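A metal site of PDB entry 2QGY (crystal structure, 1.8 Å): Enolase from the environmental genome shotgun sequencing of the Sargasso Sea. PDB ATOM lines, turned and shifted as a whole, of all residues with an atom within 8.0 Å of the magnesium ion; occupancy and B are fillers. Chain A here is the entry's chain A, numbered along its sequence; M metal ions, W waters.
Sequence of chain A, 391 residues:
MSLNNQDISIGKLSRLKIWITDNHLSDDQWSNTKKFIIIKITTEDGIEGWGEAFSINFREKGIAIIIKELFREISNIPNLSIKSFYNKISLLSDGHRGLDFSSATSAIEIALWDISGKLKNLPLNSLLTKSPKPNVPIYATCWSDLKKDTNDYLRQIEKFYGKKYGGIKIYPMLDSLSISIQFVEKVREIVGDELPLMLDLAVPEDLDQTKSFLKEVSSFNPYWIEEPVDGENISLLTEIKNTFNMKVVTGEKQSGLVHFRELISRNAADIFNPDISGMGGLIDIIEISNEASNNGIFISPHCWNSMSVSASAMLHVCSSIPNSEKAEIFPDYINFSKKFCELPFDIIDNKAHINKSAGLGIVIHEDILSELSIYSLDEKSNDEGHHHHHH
Water W3 bridges OE2 of Glu 252 and OH of Tyr 171. Water W1 bridges the side-chain carboxylate of Asp 200 and the side-chain carboxylate of Glu 227. Water W2 bridges the side-chain hydroxyl of Tyr 171 (2.8 Å) and the side-chain amino group of Lys 169 (2.9 Å).
Residues that only touch the magnesium ion: Tyr 171.
The magnesium ion is bound by OE1 of Glu 252, 2.0 Å away. The side-chain carboxylate (OD2) of Asp 200 binds the magnesium ion (2.0 Å). Water W3 is bound to the magnesium ion (2.0 Å). The magnesium ion is bound by the side-chain carboxylate (OE2) of Glu 226, at 2.0 Å. Water W1 is bound to the magnesium ion. Water W2 is bound to the magnesium ion (2.1 Å). The magnesium ion has six donor atoms within binding distance.
The side-chain carboxylate (OE2) of Glu 226 sits close to the side-chain amide nitrogen (ND2) of Asn 273 (3.1 Å). The backbone NH (N) of Asp 200 sits at hydrogen-bond distance from the backbone carbonyl oxygen (O) of Ile 170, at 2.8 Å. O of Glu 226 is in hydrogen-bond range of N of Leu 201, 2.9 Å away. The side-chain carboxylate of Glu 226 is in salt-bridge range of the side-chain amino group of Lys 169. The backbone NH (N) of Glu 252 is in hydrogen-bond range of the side-chain amide oxygen (OD1) of Asn 273, 2.9 Å away. The backbone carbonyl oxygen of Leu 199 lies within hydrogen-bond range of the backbone NH of Glu 226, 2.8 Å away. The side-chain carboxylate (OE2) of Glu 252 lies within hydrogen-bond range of a ring nitrogen (NE2) of His 302, at 3.4 Å. OE1 of Glu 226 is in hydrogen-bond range of NE1 of Trp 224 (3.1 Å).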
ATOM      1  N   TYR A 139     -28.342 -17.444  10.160  1.00  0.00           N
ATOM      2  CA  TYR A 139     -26.956 -17.072  10.356  1.00  0.00           C
ATOM      3  C   TYR A 139     -26.974 -15.625  10.834  1.00  0.00           C
ATOM      4  O   TYR A 139     -27.963 -14.906  10.647  1.00  0.00           O
ATOM      5  CB  TYR A 139     -26.146 -17.232   9.050  1.00  0.00           C
ATOM      6  CG  TYR A 139     -26.433 -16.156   8.014  1.00  0.00           C
ATOM      7  CD1 TYR A 139     -25.690 -14.972   7.982  1.00  0.00           C
ATOM      8  CD2 TYR A 139     -27.482 -16.302   7.091  1.00  0.00           C
ATOM      9  CE1 TYR A 139     -25.974 -13.939   7.036  1.00  0.00           C
ATOM     10  CE2 TYR A 139     -27.769 -15.304   6.149  1.00  0.00           C
ATOM     11  CZ  TYR A 139     -27.021 -14.130   6.138  1.00  0.00           C
ATOM     12  OH  TYR A 139     -27.299 -13.156   5.198  1.00  0.00           O
ATOM     13  N   THR A 141     -25.254 -11.791  11.006  1.00  0.00           N
ATOM     14  CA  THR A 141     -24.425 -10.819  10.308  1.00  0.00           C
ATOM     15  C   THR A 141     -23.721  -9.924  11.309  1.00  0.00           C
ATOM     16  O   THR A 141     -24.346  -9.402  12.231  1.00  0.00           O
ATOM     17  CB  THR A 141     -25.265  -9.974   9.335  1.00  0.00           C
ATOM     18  OG1 THR A 141     -25.726 -10.834   8.289  1.00  0.00           O
ATOM     19  CG2 THR A 141     -24.466  -8.847   8.724  1.00  0.00           C
ATOM     20  N   LYS A 169     -21.767 -14.066   9.075  1.00  0.00           N
ATOM     21  CA  LYS A 169     -21.363 -13.293   7.894  1.00  0.00           C
ATOM     22  C   LYS A 169     -20.517 -12.070   8.282  1.00  0.00           C
ATOM     23  O   LYS A 169     -20.903 -11.296   9.140  1.00  0.00           O
ATOM     24  CB  LYS A 169     -22.585 -12.899   7.034  1.00  0.00           C
ATOM     25  CG  LYS A 169     -22.162 -12.262   5.728  1.00  0.00           C
ATOM     26  CD  LYS A 169     -23.310 -12.054   4.735  1.00  0.00           C
ATOM     27  CE  LYS A 169     -24.315 -10.982   5.217  1.00  0.00           C
ATOM     28  NZ  LYS A 169     -25.561 -10.949   4.344  1.00  0.00           N
ATOM     29  N   ILE A 170     -19.331 -11.948   7.684  1.00  0.00           N
ATOM     30  CA  ILE A 170     -18.457 -10.802   7.922  1.00  0.00           C
ATOM     31  C   ILE A 170     -18.215  -9.967   6.670  1.00  0.00           C
ATOM     32  O   ILE A 170     -18.541 -10.402   5.536  1.00  0.00           O
ATOM     33  CB  ILE A 170     -17.095 -11.259   8.503  1.00  0.00           C
ATOM     34  CG1 ILE A 170     -16.432 -12.232   7.525  1.00  0.00           C
ATOM     35  CG2 ILE A 170     -17.296 -11.925   9.895  1.00  0.00           C
ATOM     36  CD1 ILE A 170     -14.964 -12.501   7.807  1.00  0.00           C
ATOM     37  N   TYR A 171     -17.647  -8.776   6.855  1.00  0.00           N
ATOM     38  CA  TYR A 171     -17.347  -7.868   5.766  1.00  0.00           C
ATOM     39  C   TYR A 171     -15.839  -7.660   5.735  1.00  0.00           C
ATOM     40  O   TYR A 171     -15.311  -6.759   6.403  1.00  0.00           O
ATOM     41  CB  TYR A 171     -18.085  -6.525   5.963  1.00  0.00           C
ATOM     42  CG  TYR A 171     -19.594  -6.608   5.778  1.00  0.00           C
ATOM     43  CD1 TYR A 171     -20.213  -5.998   4.682  1.00  0.00           C
ATOM     44  CD2 TYR A 171     -20.378  -7.260   6.707  1.00  0.00           C
ATOM     45  CE1 TYR A 171     -21.632  -6.081   4.515  1.00  0.00           C
ATOM     46  CE2 TYR A 171     -21.775  -7.339   6.541  1.00  0.00           C
ATOM     47  CZ  TYR A 171     -22.367  -6.754   5.442  1.00  0.00           C
ATOM     48  OH  TYR A 171     -23.754  -6.821   5.304  1.00  0.00           O
ATOM     49  N   LEU A 199     -19.005 -14.288   3.456  1.00  0.00           N
ATOM     50  CA  LEU A 199     -18.215 -13.104   3.240  1.00  0.00           C
ATOM     51  C   LEU A 199     -19.021 -12.157   2.373  1.00  0.00           C
ATOM     52  O   LEU A 199     -19.394 -12.494   1.257  1.00  0.00           O
ATOM     53  CB  LEU A 199     -16.867 -13.447   2.548  1.00  0.00           C
ATOM     54  CG  LEU A 199     -15.911 -14.470   3.214  1.00  0.00           C
ATOM     55  CD1 LEU A 199     -14.600 -14.628   2.405  1.00  0.00           C
ATOM     56  CD2 LEU A 199     -15.602 -14.121   4.662  1.00  0.00           C
ATOM     57  N   ASP A 200     -19.294 -10.973   2.903  1.00  0.00           N
ATOM     58  CA  ASP A 200     -19.992  -9.963   2.159  1.00  0.00           C
ATOM     59  C   ASP A 200     -18.991  -8.959   1.667  1.00  0.00           C
ATOM     60  O   ASP A 200     -18.443  -8.175   2.441  1.00  0.00           O
ATOM     61  CB  ASP A 200     -21.098  -9.307   3.009  1.00  0.00           C
ATOM     62  CG  ASP A 200     -22.043  -8.458   2.171  1.00  0.00           C
ATOM     63  OD1 ASP A 200     -21.608  -7.923   1.139  1.00  0.00           O
ATOM     64  OD2 ASP A 200     -23.232  -8.329   2.569  1.00  0.00           O
ATOM     65  N   LEU A 201     -18.692  -9.000   0.370  1.00  0.00           N
ATOM     66  CA  LEU A 201     -17.739  -8.045  -0.225  1.00  0.00           C
ATOM     67  C   LEU A 201     -18.291  -6.643  -0.469  1.00  0.00           C
ATOM     68  O   LEU A 201     -17.514  -5.709  -0.673  1.00  0.00           O
ATOM     69  CB  LEU A 201     -17.147  -8.577  -1.523  1.00  0.00           C
ATOM     70  CG  LEU A 201     -16.520  -9.984  -1.443  1.00  0.00           C
ATOM     71  CD1 LEU A 201     -15.617 -10.254  -2.678  1.00  0.00           C
ATOM     72  CD2 LEU A 201     -15.794 -10.209  -0.141  1.00  0.00           C
ATOM     73  N   ALA A 202     -19.618  -6.502  -0.452  1.00  0.00           N
ATOM     74  CA  ALA A 202     -20.244  -5.172  -0.468  1.00  0.00           C
ATOM     75  C   ALA A 202     -19.885  -4.330  -1.716  1.00  0.00           C
ATOM     76  O   ALA A 202     -19.702  -3.117  -1.630  1.00  0.00           O
ATOM     77  CB  ALA A 202     -19.913  -4.407   0.836  1.00  0.00           C
ATOM     78  N   VAL A 203     -19.745  -5.006  -2.860  1.00  0.00           N
ATOM     79  CA  VAL A 203     -19.505  -4.387  -4.174  1.00  0.00           C
ATOM     80  C   VAL A 203     -18.232  -3.523  -4.147  1.00  0.00           C
ATOM     81  O   VAL A 203     -18.319  -2.292  -4.186  1.00  0.00           O
ATOM     82  CB  VAL A 203     -20.730  -3.591  -4.675  1.00  0.00           C
ATOM     83  CG1 VAL A 203     -20.531  -3.142  -6.129  1.00  0.00           C
ATOM     84  CG2 VAL A 203     -22.018  -4.421  -4.559  1.00  0.00           C
ATOM     85  N   TRP A 224     -20.115 -18.674   1.376  1.00  0.00           N
ATOM     86  CA  TRP A 224     -20.547 -17.951   0.164  1.00  0.00           C
ATOM     87  C   TRP A 224     -19.873 -16.624   0.066  1.00  0.00           C
ATOM     88  O   TRP A 224     -19.269 -16.157   1.032  1.00  0.00           O
ATOM     89  CB  TRP A 224     -22.071 -17.839   0.065  1.00  0.00           C
ATOM     90  CG  TRP A 224     -22.816 -16.824   0.932  1.00  0.00           C
ATOM     91  CD1 TRP A 224     -22.561 -15.469   1.102  1.00  0.00           C
ATOM     92  CD2 TRP A 224     -24.030 -17.079   1.626  1.00  0.00           C
ATOM     93  NE1 TRP A 224     -23.533 -14.906   1.909  1.00  0.00           N
ATOM     94  CE2 TRP A 224     -24.440 -15.877   2.251  1.00  0.00           C
ATOM     95  CE3 TRP A 224     -24.809 -18.232   1.798  1.00  0.00           C
ATOM     96  CZ2 TRP A 224     -25.602 -15.794   3.022  1.00  0.00           C
ATOM     97  CZ3 TRP A 224     -25.972 -18.149   2.569  1.00  0.00           C
ATOM     98  CH2 TRP A 224     -26.357 -16.927   3.166  1.00  0.00           C
ATOM     99  N   GLU A 226     -20.723 -12.811  -1.154  1.00  0.00           N
ATOM    100  CA  GLU A 226     -21.898 -12.005  -1.394  1.00  0.00           C
ATOM    101  C   GLU A 226     -21.512 -10.676  -2.052  1.00  0.00           C
ATOM    102  O   GLU A 226     -20.534 -10.023  -1.643  1.00  0.00           O
ATOM    103  CB  GLU A 226     -22.621 -11.802  -0.064  1.00  0.00           C
ATOM    104  CG  GLU A 226     -23.809 -10.914  -0.136  1.00  0.00           C
ATOM    105  CD  GLU A 226     -24.620 -10.932   1.157  1.00  0.00           C
ATOM    106  OE1 GLU A 226     -24.698 -11.989   1.829  1.00  0.00           O
ATOM    107  OE2 GLU A 226     -25.215  -9.902   1.454  1.00  0.00           O
ATOM    108  N   GLU A 227     -22.253 -10.310  -3.110  1.00  0.00           N
ATOM    109  CA  GLU A 227     -22.046  -9.073  -3.837  1.00  0.00           C
ATOM    110  C   GLU A 227     -20.568  -8.786  -4.198  1.00  0.00           C
ATOM    111  O   GLU A 227     -20.070  -7.715  -3.925  1.00  0.00           O
ATOM    112  CB  GLU A 227     -22.660  -7.896  -3.080  1.00  0.00           C
ATOM    113  CG  GLU A 227     -24.174  -7.990  -2.938  1.00  0.00           C
ATOM    114  CD  GLU A 227     -24.784  -6.630  -3.081  1.00  0.00           C
ATOM    115  OE1 GLU A 227     -24.668  -5.877  -2.093  1.00  0.00           O
ATOM    116  OE2 GLU A 227     -25.304  -6.304  -4.195  1.00  0.00           O
ATOM    117  N   VAL A 249     -23.617 -14.891  -4.247  1.00  0.00           N
ATOM    118  CA  VAL A 249     -24.906 -14.404  -3.755  1.00  0.00           C
ATOM    119  C   VAL A 249     -25.147 -12.986  -4.291  1.00  0.00           C
ATOM    120  O   VAL A 249     -24.262 -12.159  -4.213  1.00  0.00           O
ATOM    121  CB  VAL A 249     -24.927 -14.347  -2.213  1.00  0.00           C
ATOM    122  CG1 VAL A 249     -26.366 -13.933  -1.738  1.00  0.00           C
ATOM    123  CG2 VAL A 249     -24.622 -15.744  -1.613  1.00  0.00           C
ATOM    124  N   THR A 250     -26.336 -12.694  -4.802  1.00  0.00           N
ATOM    125  CA  THR A 250     -26.643 -11.337  -5.258  1.00  0.00           C
ATOM    126  C   THR A 250     -28.141 -11.134  -5.101  1.00  0.00           C
ATOM    127  O   THR A 250     -28.847 -12.120  -4.991  1.00  0.00           O
ATOM    128  CB  THR A 250     -26.236 -11.085  -6.752  1.00  0.00           C
ATOM    129  OG1 THR A 250     -26.408  -9.683  -7.095  1.00  0.00           O
ATOM    130  CG2 THR A 250     -27.054 -11.926  -7.698  1.00  0.00           C
ATOM    131  N   GLY A 251     -28.595  -9.879  -5.080  1.00  0.00           N
ATOM    132  CA  GLY A 251     -30.037  -9.651  -5.160  1.00  0.00           C
ATOM    133  C   GLY A 251     -30.529  -8.624  -4.160  1.00  0.00           C
ATOM    134  O   GLY A 251     -31.533  -7.977  -4.402  1.00  0.00           O
ATOM    135  N   GLU A 252     -29.817  -8.468  -3.039  1.00  0.00           N
ATOM    136  CA  GLU A 252     -30.260  -7.553  -1.977  1.00  0.00           C
ATOM    137  C   GLU A 252     -30.565  -6.119  -2.418  1.00  0.00           C
ATOM    138  O   GLU A 252     -31.425  -5.468  -1.827  1.00  0.00           O
ATOM    139  CB  GLU A 252     -29.252  -7.554  -0.830  1.00  0.00           C
ATOM    140  CG  GLU A 252     -27.931  -6.935  -1.136  1.00  0.00           C
ATOM    141  CD  GLU A 252     -27.115  -6.756   0.142  1.00  0.00           C
ATOM    142  OE1 GLU A 252     -26.605  -7.770   0.622  1.00  0.00           O
ATOM    143  OE2 GLU A 252     -27.040  -5.635   0.696  1.00  0.00           O
ATOM    144  N   LYS A 253     -29.875  -5.612  -3.432  1.00  0.00           N
ATOM    145  CA  LYS A 253     -30.107  -4.212  -3.832  1.00  0.00           C
ATOM    146  C   LYS A 253     -31.016  -4.103  -5.071  1.00  0.00           C
ATOM    147  O   LYS A 253     -31.156  -3.018  -5.638  1.00  0.00           O
ATOM    148  CB  LYS A 253     -28.749  -3.505  -4.049  1.00  0.00           C
ATOM    149  CG  LYS A 253     -27.963  -3.447  -2.725  1.00  0.00           C
ATOM    150  CD  LYS A 253     -26.926  -2.359  -2.587  1.00  0.00           C
ATOM    151  CE  LYS A 253     -26.130  -2.635  -1.312  1.00  0.00           C
ATOM    152  NZ  LYS A 253     -25.232  -1.536  -0.879  1.00  0.00           N
ATOM    153  N   ASN A 273     -30.432 -13.087  -2.659  1.00  0.00           N
ATOM    154  CA  ASN A 273     -30.766 -12.548  -1.346  1.00  0.00           C
ATOM    155  C   ASN A 273     -31.570 -11.230  -1.459  1.00  0.00           C
ATOM    156  O   ASN A 273     -31.195 -10.237  -0.876  1.00  0.00           O
ATOM    157  CB  ASN A 273     -29.499 -12.399  -0.473  1.00  0.00           C
ATOM    158  CG  ASN A 273     -28.567 -11.271  -0.960  1.00  0.00           C
ATOM    159  OD1 ASN A 273     -28.540 -10.948  -2.141  1.00  0.00           O
ATOM    160  ND2 ASN A 273     -27.840 -10.645  -0.027  1.00  0.00           N
ATOM    161  N   HIS A 302     -32.516 -11.344   2.460  1.00  0.00           N
ATOM    162  CA  HIS A 302     -31.703 -10.360   3.135  1.00  0.00           C
ATOM    163  C   HIS A 302     -32.695  -9.760   4.137  1.00  0.00           C
ATOM    164  O   HIS A 302     -33.886  -9.708   3.874  1.00  0.00           O
ATOM    165  CB  HIS A 302     -31.243  -9.347   2.084  1.00  0.00           C
ATOM    166  CG  HIS A 302     -30.534  -8.123   2.609  1.00  0.00           C
ATOM    167  ND1 HIS A 302     -31.199  -6.944   2.862  1.00  0.00           N
ATOM    168  CD2 HIS A 302     -29.218  -7.855   2.784  1.00  0.00           C
ATOM    169  CE1 HIS A 302     -30.342  -6.013   3.221  1.00  0.00           C
ATOM    170  NE2 HIS A 302     -29.125  -6.540   3.191  1.00  0.00           N
ATOM    171  N   TRP A 304     -32.005  -6.641   6.506  1.00  0.00           N
ATOM    172  CA  TRP A 304     -31.462  -5.526   7.247  1.00  0.00           C
ATOM    173  C   TRP A 304     -32.652  -4.610   7.565  1.00  0.00           C
ATOM    174  O   TRP A 304     -32.910  -3.596   6.914  1.00  0.00           O
ATOM    175  CB  TRP A 304     -30.320  -4.829   6.506  1.00  0.00           C
ATOM    176  CG  TRP A 304     -29.634  -3.774   7.323  1.00  0.00           C
ATOM    177  CD1 TRP A 304     -29.334  -3.822   8.646  1.00  0.00           C
ATOM    178  CD2 TRP A 304     -29.223  -2.478   6.861  1.00  0.00           C
ATOM    179  NE1 TRP A 304     -28.733  -2.638   9.043  1.00  0.00           N
ATOM    180  CE2 TRP A 304     -28.637  -1.811   7.968  1.00  0.00           C
ATOM    181  CE3 TRP A 304     -29.282  -1.839   5.625  1.00  0.00           C
ATOM    182  CZ2 TRP A 304     -28.117  -0.513   7.860  1.00  0.00           C
ATOM    183  CZ3 TRP A 304     -28.742  -0.543   5.511  1.00  0.00           C
ATOM    184  CH2 TRP A 304     -28.186   0.098   6.637  1.00  0.00           C
ATOM    185  N   GLU A 328     -31.171 -14.480   7.345  1.00  0.00           N
ATOM    186  CA  GLU A 328     -30.278 -13.508   7.942  1.00  0.00           C
ATOM    187  C   GLU A 328     -30.851 -12.879   9.232  1.00  0.00           C
ATOM    188  O   GLU A 328     -32.015 -12.408   9.246  1.00  0.00           O
ATOM    189  CB  GLU A 328     -30.016 -12.359   6.951  1.00  0.00           C
ATOM    190  CG  GLU A 328     -29.073 -11.327   7.518  1.00  0.00           C
ATOM    191  CD  GLU A 328     -28.626 -10.300   6.488  1.00  0.00           C
ATOM    192  OE1 GLU A 328     -29.436  -9.979   5.593  1.00  0.00           O
ATOM    193  OE2 GLU A 328     -27.464  -9.852   6.544  1.00  0.00           O
ATOM    194  N   PHE A 330     -29.689 -10.058  12.517  1.00  0.00           N
ATOM    195  CA  PHE A 330     -28.756  -9.106  13.115  1.00  0.00           C
ATOM    196  C   PHE A 330     -28.932  -9.275  14.610  1.00  0.00           C
ATOM    197  O   PHE A 330     -29.932  -8.818  15.160  1.00  0.00           O
ATOM    198  CB  PHE A 330     -29.084  -7.671  12.696  1.00  0.00           C
ATOM    199  CG  PHE A 330     -28.580  -7.328  11.347  1.00  0.00           C
ATOM    200  CD1 PHE A 330     -27.431  -6.568  11.183  1.00  0.00           C
ATOM    201  CD2 PHE A 330     -29.254  -7.781  10.218  1.00  0.00           C
ATOM    202  CE1 PHE A 330     -26.961  -6.262   9.906  1.00  0.00           C
ATOM    203  CE2 PHE A 330     -28.791  -7.479   8.921  1.00  0.00           C
ATOM    204  CZ  PHE A 330     -27.627  -6.730   8.773  1.00  0.00           C
HETATM  205 MG    MG M   1     -24.972  -7.892   1.689  1.00  0.00          MG
HETATM  206  O   HOH W   1     -23.893  -7.170   0.087  1.00  0.00           O
HETATM  207  O   HOH W   2     -25.704  -8.110   3.685  1.00  0.00           O
HETATM  208  O   HOH W   3     -24.920  -5.967   2.254  1.00  0.00           O
